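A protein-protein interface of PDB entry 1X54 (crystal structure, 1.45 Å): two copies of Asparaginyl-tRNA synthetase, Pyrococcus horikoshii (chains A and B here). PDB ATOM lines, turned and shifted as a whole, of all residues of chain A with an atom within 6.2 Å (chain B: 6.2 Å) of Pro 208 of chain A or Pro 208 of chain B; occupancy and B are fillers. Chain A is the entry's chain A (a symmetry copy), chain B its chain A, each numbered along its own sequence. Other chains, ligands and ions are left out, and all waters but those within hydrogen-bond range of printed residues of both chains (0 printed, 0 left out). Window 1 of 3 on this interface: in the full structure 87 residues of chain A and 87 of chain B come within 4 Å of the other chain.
Ile 161 of chain A touches Pro 208 of chain B, and with the chains exchanged Pro 208 of chain A touches Ile 161 of chain B. Ile 161 of chain A touches Phe 210 of chain B, and with the chains exchanged Phe 210 of chain A touches Ile 161 of chain B. Ile 161 of chain A touches Glu 223 of chain B, and with the chains exchanged Glu 223 of chain A touches Ile 161 of chain B. Pro 208 of chain A touches its own counterpart, Pro 208 of chain B. 12 positions are printed for both chains. Of the 9 pairs that touch across the chains among the printed residues, 9 have their exchanged pair printed and touching as well.
Of chain B, only Ile 161 (3.8 Å) and Pro 208 (3.7 Å) come within 4 Å of Pro 208 of chain A. Of chain A, only Ile 161 and Pro 208 come within 4 Å of Pro 208 of chain B. Of the printed residues of chain B, Phe 210 of chain A touches Ile 161 (3.7 Å). Of the printed residues of chain B, Trp 225 of chain A touches Leu 206. Ser 188 of chain B touches none of the printed residues of chain A. Ser 209 of chain B touches none of the printed residues of chain A. The nearest residue of chain B that does not touch Pro 208 of chain A is Trp 225 of chain B (4.6 Å). The nearest residue of chain A that does not touch Pro 208 of chain B is Trp 225 of chain A (4.6 Å).
Among the printed residues, pairs that only touch across the chains: Pro 208 of chain A with Pro 208 of chain B (3.7 Å), Ile 161 of chain A with Phe 210 of chain B (3.7 Å), Phe 210 of chain A with Ile 161 of chain B (3.7 Å), Pro 208 of chain A with Ile 161 of chain B (3.8 Å), Ile 161 of chain A with Pro 208 of chain B (3.8 Å), Leu 206 of chain A with Trp 225 of chain B (3.8 Å) and Trp 225 of chain A with Leu 206 of chain B (3.8 Å).
OE2 of Glu 223 of chain B lies within hydrogen-bond range of N of Ile 161 of chain A, 3.0 Å away. The backbone NH (N) of Ile 161 of chain B lies within hydrogen-bond range of the side-chain carboxylate (OE2) of Glu 223 of chain A, at 3.0 Å.
The backbone carbonyl oxygen (O) of Ser 186 of chain A is in hydrogen-bond range of the backbone NH (N) of Phe 210 of chain A. O of Ile 161 of chain A sits at hydrogen-bond distance from N of Ser 186 of chain A (2.7 Å). O of Ile 161 of chain B sits at hydrogen-bond distance from N of Ser 186 of chain B, at 2.7 Å. N of Phe 210 of chain B lies within hydrogen-bond range of O of Ser 186 of chain B.
Of the 12 printed residues of chain A, 6 touch a printed residue of chain B. Hydrophobic or aromatic side chains of chain A that line the printed part of chain B: Ile 161, Pro 208, Phe 210 and Trp 225. Along chain A the printed residues that touch a printed residue of chain B span positions 161 to 225. Hydrophobic or aromatic side chains of chain B within 4 Å of the printed part of chain A: Ile 161, Pro 208, Phe 210 and Trp 225. Among the printed residues, 9 pairs touch across the chains. Among the printed residues, no Asp or Glu carboxylate lies within 4 Å of a Lys or Arg side-chain nitrogen of the other chain.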
ATOM      1  N   ILE A 161       5.296  -1.746 -28.762  1.00  0.00           N
ATOM      2  CA  ILE A 161       4.964  -1.296 -27.419  1.00  0.00           C
ATOM      3  C   ILE A 161       4.186   0.019 -27.430  1.00  0.00           C
ATOM      4  O   ILE A 161       3.258   0.192 -26.639  1.00  0.00           O
ATOM      5  CB  ILE A 161       6.239  -1.165 -26.559  1.00  0.00           C
ATOM      6  CG1 ILE A 161       7.084  -2.463 -26.641  1.00  0.00           C
ATOM      7  CG2 ILE A 161       5.880  -0.728 -25.141  1.00  0.00           C
ATOM      8  CD1 ILE A 161       6.364  -3.756 -26.253  1.00  0.00           C
ATOM      9  N   SER A 186       1.583  -0.329 -24.532  1.00  0.00           N
ATOM     10  CA  SER A 186       0.864  -1.591 -24.710  1.00  0.00           C
ATOM     11  C   SER A 186       0.537  -2.303 -23.404  1.00  0.00           C
ATOM     12  O   SER A 186       1.409  -2.530 -22.575  1.00  0.00           O
ATOM     13  CB  SER A 186       1.708  -2.531 -25.567  1.00  0.00           C
ATOM     14  OG  SER A 186       1.081  -3.811 -25.681  1.00  0.00           O
ATOM     15  N   SER A 188      -0.723  -5.348 -23.774  1.00  0.00           N
ATOM     16  CA  SER A 188      -0.761  -6.705 -24.310  1.00  0.00           C
ATOM     17  C   SER A 188      -0.515  -6.609 -25.811  1.00  0.00           C
ATOM     18  O   SER A 188      -1.047  -5.701 -26.468  1.00  0.00           O
ATOM     19  CB  SER A 188      -2.135  -7.338 -24.068  1.00  0.00           C
ATOM     20  OG  SER A 188      -2.318  -8.477 -24.885  1.00  0.00           O
ATOM     21  N   LEU A 206       7.344 -12.288 -26.382  1.00  0.00           N
ATOM     22  CA  LEU A 206       7.594 -11.981 -24.990  1.00  0.00           C
ATOM     23  C   LEU A 206       7.909 -10.497 -24.898  1.00  0.00           C
ATOM     24  O   LEU A 206       8.926 -10.036 -25.414  1.00  0.00           O
ATOM     25  CB  LEU A 206       8.749 -12.836 -24.441  1.00  0.00           C
ATOM     26  CG  LEU A 206       9.174 -12.554 -22.997  1.00  0.00           C
ATOM     27  CD1 LEU A 206       8.025 -12.843 -22.006  1.00  0.00           C
ATOM     28  CD2 LEU A 206      10.448 -13.365 -22.653  1.00  0.00           C
ATOM     29  N   THR A 207       7.011  -9.740 -24.261  1.00  0.00           N
ATOM     30  CA  THR A 207       7.158  -8.280 -24.229  1.00  0.00           C
ATOM     31  C   THR A 207       6.830  -7.773 -22.854  1.00  0.00           C
ATOM     32  O   THR A 207       6.124  -8.425 -22.090  1.00  0.00           O
ATOM     33  CB  THR A 207       6.221  -7.556 -25.232  1.00  0.00           C
ATOM     34  OG1 THR A 207       4.864  -7.895 -24.926  1.00  0.00           O
ATOM     35  CG2 THR A 207       6.484  -8.027 -26.681  1.00  0.00           C
ATOM     36  N   PRO A 208       7.336  -6.589 -22.538  1.00  0.00           N
ATOM     37  CA  PRO A 208       6.883  -5.897 -21.343  1.00  0.00           C
ATOM     38  C   PRO A 208       5.516  -5.299 -21.642  1.00  0.00           C
ATOM     39  O   PRO A 208       5.307  -4.686 -22.707  1.00  0.00           O
ATOM     40  CB  PRO A 208       7.950  -4.811 -21.137  1.00  0.00           C
ATOM     41  CG  PRO A 208       8.425  -4.502 -22.534  1.00  0.00           C
ATOM     42  CD  PRO A 208       8.376  -5.848 -23.276  1.00  0.00           C
ATOM     43  N   SER A 209       4.599  -5.513 -20.700  1.00  0.00           N
ATOM     44  CA  SER A 209       3.259  -4.941 -20.760  1.00  0.00           C
ATOM     45  C   SER A 209       3.064  -3.986 -19.594  1.00  0.00           C
ATOM     46  O   SER A 209       3.671  -4.135 -18.549  1.00  0.00           O
ATOM     47  CB  SER A 209       2.181  -6.043 -20.723  1.00  0.00           C
ATOM     48  OG  SER A 209       2.190  -6.847 -21.900  1.00  0.00           O
ATOM     49  N   PHE A 210       2.200  -3.006 -19.798  1.00  0.00           N
ATOM     50  CA  PHE A 210       2.118  -1.866 -18.879  1.00  0.00           C
ATOM     51  C   PHE A 210       0.698  -1.706 -18.446  1.00  0.00           C
ATOM     52  O   PHE A 210      -0.199  -1.679 -19.286  1.00  0.00           O
ATOM     53  CB  PHE A 210       2.665  -0.596 -19.545  1.00  0.00           C
ATOM     54  CG  PHE A 210       4.093  -0.747 -19.982  1.00  0.00           C
ATOM     55  CD1 PHE A 210       5.135  -0.400 -19.126  1.00  0.00           C
ATOM     56  CD2 PHE A 210       4.392  -1.275 -21.228  1.00  0.00           C
ATOM     57  CE1 PHE A 210       6.471  -0.588 -19.512  1.00  0.00           C
ATOM     58  CE2 PHE A 210       5.718  -1.483 -21.622  1.00  0.00           C
ATOM     59  CZ  PHE A 210       6.760  -1.116 -20.769  1.00  0.00           C
ATOM     60  N   GLU A 223       4.413  -2.797 -14.595  1.00  0.00           N
ATOM     61  CA  GLU A 223       5.171  -3.254 -15.762  1.00  0.00           C
ATOM     62  C   GLU A 223       5.482  -4.725 -15.501  1.00  0.00           C
ATOM     63  O   GLU A 223       5.981  -5.074 -14.434  1.00  0.00           O
ATOM     64  CB  GLU A 223       6.473  -2.444 -15.856  1.00  0.00           C
ATOM     65  CG  GLU A 223       7.509  -2.920 -16.863  1.00  0.00           C
ATOM     66  CD  GLU A 223       8.775  -2.105 -16.735  1.00  0.00           C
ATOM     67  OE1 GLU A 223       8.680  -0.859 -16.866  1.00  0.00           O
ATOM     68  OE2 GLU A 223       9.844  -2.699 -16.471  1.00  0.00           O
ATOM     69  N   PHE A 224       5.148  -5.593 -16.447  1.00  0.00           N
ATOM     70  CA  PHE A 224       5.416  -7.020 -16.244  1.00  0.00           C
ATOM     71  C   PHE A 224       5.766  -7.680 -17.573  1.00  0.00           C
ATOM     72  O   PHE A 224       5.499  -7.103 -18.637  1.00  0.00           O
ATOM     73  CB  PHE A 224       4.227  -7.725 -15.557  1.00  0.00           C
ATOM     74  CG  PHE A 224       3.013  -7.885 -16.428  1.00  0.00           C
ATOM     75  CD1 PHE A 224       2.814  -9.088 -17.131  1.00  0.00           C
ATOM     76  CD2 PHE A 224       2.048  -6.873 -16.524  1.00  0.00           C
ATOM     77  CE1 PHE A 224       1.682  -9.260 -17.936  1.00  0.00           C
ATOM     78  CE2 PHE A 224       0.915  -7.047 -17.342  1.00  0.00           C
ATOM     79  CZ  PHE A 224       0.739  -8.242 -18.037  1.00  0.00           C
ATOM     80  N   TRP A 225       6.360  -8.873 -17.501  1.00  0.00           N
ATOM     81  CA  TRP A 225       6.732  -9.599 -18.715  1.00  0.00           C
ATOM     82  C   TRP A 225       5.621 -10.575 -19.080  1.00  0.00           C
ATOM     83  O   TRP A 225       5.127 -11.332 -18.231  1.00  0.00           O
ATOM     84  CB  TRP A 225       8.110 -10.262 -18.555  1.00  0.00           C
ATOM     85  CG  TRP A 225       9.182  -9.195 -18.681  1.00  0.00           C
ATOM     86  CD1 TRP A 225       9.637  -8.339 -17.697  1.00  0.00           C
ATOM     87  CD2 TRP A 225       9.830  -8.783 -19.893  1.00  0.00           C
ATOM     88  NE1 TRP A 225      10.545  -7.455 -18.229  1.00  0.00           N
ATOM     89  CE2 TRP A 225      10.701  -7.720 -19.570  1.00  0.00           C
ATOM     90  CE3 TRP A 225       9.794  -9.244 -21.223  1.00  0.00           C
ATOM     91  CZ2 TRP A 225      11.518  -7.107 -20.520  1.00  0.00           C
ATOM     92  CZ3 TRP A 225      10.608  -8.638 -22.169  1.00  0.00           C
ATOM     93  CH2 TRP A 225      11.456  -7.574 -21.812  1.00  0.00           C
ATOM     94  N   HIS A 226       5.227 -10.521 -20.347  1.00  0.00           N
ATOM     95  CA  HIS A 226       3.987 -11.087 -20.808  1.00  0.00           C
ATOM     96  C   HIS A 226       4.311 -12.023 -21.985  1.00  0.00           C
ATOM     97  O   HIS A 226       4.776 -11.563 -23.026  1.00  0.00           O
ATOM     98  CB  HIS A 226       3.119  -9.921 -21.279  1.00  0.00           C
ATOM     99  CG  HIS A 226       1.656 -10.225 -21.352  1.00  0.00           C
ATOM    100  ND1 HIS A 226       0.733  -9.252 -21.656  1.00  0.00           N
ATOM    101  CD2 HIS A 226       0.947 -11.372 -21.156  1.00  0.00           C
ATOM    102  CE1 HIS A 226      -0.482  -9.782 -21.649  1.00  0.00           C
ATOM    103  NE2 HIS A 226      -0.382 -11.065 -21.354  1.00  0.00           N
ATOM    104  N   ILE B 161      11.743  -1.135 -18.107  1.00  0.00           N
ATOM    105  CA  ILE B 161      11.508  -0.189 -19.188  1.00  0.00           C
ATOM    106  C   ILE B 161      11.185   1.210 -18.666  1.00  0.00           C
ATOM    107  O   ILE B 161      11.640   2.201 -19.238  1.00  0.00           O
ATOM    108  CB  ILE B 161      10.385  -0.695 -20.118  1.00  0.00           C
ATOM    109  CG1 ILE B 161      10.660  -2.157 -20.556  1.00  0.00           C
ATOM    110  CG2 ILE B 161      10.170   0.284 -21.270  1.00  0.00           C
ATOM    111  CD1 ILE B 161      12.008  -2.410 -21.235  1.00  0.00           C
ATOM    112  N   SER B 186      12.940   3.647 -21.171  1.00  0.00           N
ATOM    113  CA  SER B 186      14.338   3.237 -21.307  1.00  0.00           C
ATOM    114  C   SER B 186      14.891   3.392 -22.718  1.00  0.00           C
ATOM    115  O   SER B 186      14.306   2.911 -23.680  1.00  0.00           O
ATOM    116  CB  SER B 186      14.470   1.771 -20.903  1.00  0.00           C
ATOM    117  OG  SER B 186      15.806   1.306 -21.118  1.00  0.00           O
ATOM    118  N   SER B 188      17.911   2.099 -23.165  1.00  0.00           N
ATOM    119  CA  SER B 188      18.925   1.052 -23.081  1.00  0.00           C
ATOM    120  C   SER B 188      18.872   0.479 -21.670  1.00  0.00           C
ATOM    121  O   SER B 188      18.728   1.238 -20.699  1.00  0.00           O
ATOM    122  CB  SER B 188      20.318   1.635 -23.332  1.00  0.00           C
ATOM    123  OG  SER B 188      21.326   0.743 -22.898  1.00  0.00           O
ATOM    124  N   LEU B 206      17.083  -8.801 -23.914  1.00  0.00           N
ATOM    125  CA  LEU B 206      16.517  -8.329 -25.159  1.00  0.00           C
ATOM    126  C   LEU B 206      15.273  -7.523 -24.821  1.00  0.00           C
ATOM    127  O   LEU B 206      14.289  -8.066 -24.320  1.00  0.00           O
ATOM    128  CB  LEU B 206      16.188  -9.507 -26.091  1.00  0.00           C
ATOM    129  CG  LEU B 206      15.505  -9.154 -27.415  1.00  0.00           C
ATOM    130  CD1 LEU B 206      16.407  -8.259 -28.292  1.00  0.00           C
ATOM    131  CD2 LEU B 206      15.084 -10.448 -28.156  1.00  0.00           C
ATOM    132  N   THR B 207      15.332  -6.211 -25.068  1.00  0.00           N
ATOM    133  CA  THR B 207      14.234  -5.328 -24.659  1.00  0.00           C
ATOM    134  C   THR B 207      13.954  -4.337 -25.752  1.00  0.00           C
ATOM    135  O   THR B 207      14.809  -4.054 -26.586  1.00  0.00           O
ATOM    136  CB  THR B 207      14.551  -4.526 -23.368  1.00  0.00           C
ATOM    137  OG1 THR B 207      15.727  -3.738 -23.591  1.00  0.00           O
ATOM    138  CG2 THR B 207      14.863  -5.473 -22.186  1.00  0.00           C
ATOM    139  N   PRO B 208      12.746  -3.791 -25.743  1.00  0.00           N
ATOM    140  CA  PRO B 208      12.454  -2.648 -26.592  1.00  0.00           C
ATOM    141  C   PRO B 208      13.079  -1.419 -25.949  1.00  0.00           C
ATOM    142  O   PRO B 208      12.952  -1.203 -24.729  1.00  0.00           O
ATOM    143  CB  PRO B 208      10.920  -2.582 -26.581  1.00  0.00           C
ATOM    144  CG  PRO B 208      10.544  -3.135 -25.230  1.00  0.00           C
ATOM    145  CD  PRO B 208      11.584  -4.232 -24.948  1.00  0.00           C
ATOM    146  N   SER B 209      13.770  -0.646 -26.786  1.00  0.00           N
ATOM    147  CA  SER B 209      14.363   0.623 -26.380  1.00  0.00           C
ATOM    148  C   SER B 209      13.710   1.756 -27.152  1.00  0.00           C
ATOM    149  O   SER B 209      13.238   1.575 -28.260  1.00  0.00           O
ATOM    150  CB  SER B 209      15.886   0.629 -26.623  1.00  0.00           C
ATOM    151  OG  SER B 209      16.573  -0.283 -25.769  1.00  0.00           O
ATOM    152  N   PHE B 210      13.700   2.930 -26.543  1.00  0.00           N
ATOM    153  CA  PHE B 210      12.872   4.034 -27.040  1.00  0.00           C
ATOM    154  C   PHE B 210      13.739   5.236 -27.217  1.00  0.00           C
ATOM    155  O   PHE B 210      14.478   5.598 -26.304  1.00  0.00           O
ATOM    156  CB  PHE B 210      11.700   4.301 -26.085  1.00  0.00           C
ATOM    157  CG  PHE B 210      10.823   3.098 -25.903  1.00  0.00           C
ATOM    158  CD1 PHE B 210       9.723   2.893 -26.732  1.00  0.00           C
ATOM    159  CD2 PHE B 210      11.121   2.153 -24.934  1.00  0.00           C
ATOM    160  CE1 PHE B 210       8.930   1.743 -26.598  1.00  0.00           C
ATOM    161  CE2 PHE B 210      10.350   0.993 -24.797  1.00  0.00           C
ATOM    162  CZ  PHE B 210       9.237   0.801 -25.617  1.00  0.00           C
ATOM    163  N   GLU B 223      11.291   3.205 -31.656  1.00  0.00           N
ATOM    164  CA  GLU B 223      11.198   2.021 -30.798  1.00  0.00           C
ATOM    165  C   GLU B 223      11.935   0.913 -31.544  1.00  0.00           C
ATOM    166  O   GLU B 223      11.673   0.677 -32.720  1.00  0.00           O
ATOM    167  CB  GLU B 223       9.718   1.651 -30.621  1.00  0.00           C
ATOM    168  CG  GLU B 223       9.416   0.318 -29.954  1.00  0.00           C
ATOM    169  CD  GLU B 223       7.930   0.045 -29.980  1.00  0.00           C
ATOM    170  OE1 GLU B 223       7.173   0.898 -29.453  1.00  0.00           O
ATOM    171  OE2 GLU B 223       7.523  -0.991 -30.551  1.00  0.00           O
ATOM    172  N   PHE B 224      12.884   0.263 -30.883  1.00  0.00           N
ATOM    173  CA  PHE B 224      13.629  -0.806 -31.556  1.00  0.00           C
ATOM    174  C   PHE B 224      13.991  -1.900 -30.557  1.00  0.00           C
ATOM    175  O   PHE B 224      13.930  -1.668 -29.341  1.00  0.00           O
ATOM    176  CB  PHE B 224      14.881  -0.256 -32.272  1.00  0.00           C
ATOM    177  CG  PHE B 224      15.981   0.185 -31.348  1.00  0.00           C
ATOM    178  CD1 PHE B 224      17.028  -0.702 -31.038  1.00  0.00           C
ATOM    179  CD2 PHE B 224      16.009   1.483 -30.817  1.00  0.00           C
ATOM    180  CE1 PHE B 224      18.069  -0.304 -30.191  1.00  0.00           C
ATOM    181  CE2 PHE B 224      17.053   1.876 -29.959  1.00  0.00           C
ATOM    182  CZ  PHE B 224      18.077   0.980 -29.657  1.00  0.00           C
ATOM    183  N   TRP B 225      14.357  -3.073 -31.075  1.00  0.00           N
ATOM    184  CA  TRP B 225      14.733  -4.189 -30.207  1.00  0.00           C
ATOM    185  C   TRP B 225      16.245  -4.203 -30.029  1.00  0.00           C
ATOM    186  O   TRP B 225      17.008  -4.108 -31.002  1.00  0.00           O
ATOM    187  CB  TRP B 225      14.161  -5.513 -30.740  1.00  0.00           C
ATOM    188  CG  TRP B 225      12.678  -5.567 -30.424  1.00  0.00           C
ATOM    189  CD1 TRP B 225      11.643  -4.995 -31.139  1.00  0.00           C
ATOM    190  CD2 TRP B 225      12.083  -6.110 -29.237  1.00  0.00           C
ATOM    191  NE1 TRP B 225      10.454  -5.187 -30.477  1.00  0.00           N
ATOM    192  CE2 TRP B 225      10.692  -5.889 -29.318  1.00  0.00           C
ATOM    193  CE3 TRP B 225      12.590  -6.810 -28.126  1.00  0.00           C
ATOM    194  CZ2 TRP B 225       9.805  -6.331 -28.336  1.00  0.00           C
ATOM    195  CZ3 TRP B 225      11.710  -7.254 -27.149  1.00  0.00           C
ATOM    196  CH2 TRP B 225      10.330  -7.006 -27.259  1.00  0.00           C
ATOM    197  N   HIS B 226      16.656  -4.298 -28.769  1.00  0.00           N
ATOM    198  CA  HIS B 226      17.997  -3.981 -28.355  1.00  0.00           C
ATOM    199  C   HIS B 226      18.545  -5.194 -27.582  1.00  0.00           C
ATOM    200  O   HIS B 226      18.029  -5.528 -26.517  1.00  0.00           O
ATOM    201  CB  HIS B 226      17.898  -2.765 -27.435  1.00  0.00           C
ATOM    202  CG  HIS B 226      19.174  -2.001 -27.276  1.00  0.00           C
ATOM    203  ND1 HIS B 226      19.225  -0.823 -26.568  1.00  0.00           N
ATOM    204  CD2 HIS B 226      20.440  -2.225 -27.730  1.00  0.00           C
ATOM    205  CE1 HIS B 226      20.464  -0.353 -26.586  1.00  0.00           C
ATOM    206  NE2 HIS B 226      21.222  -1.183 -27.278  1.00  0.00           N
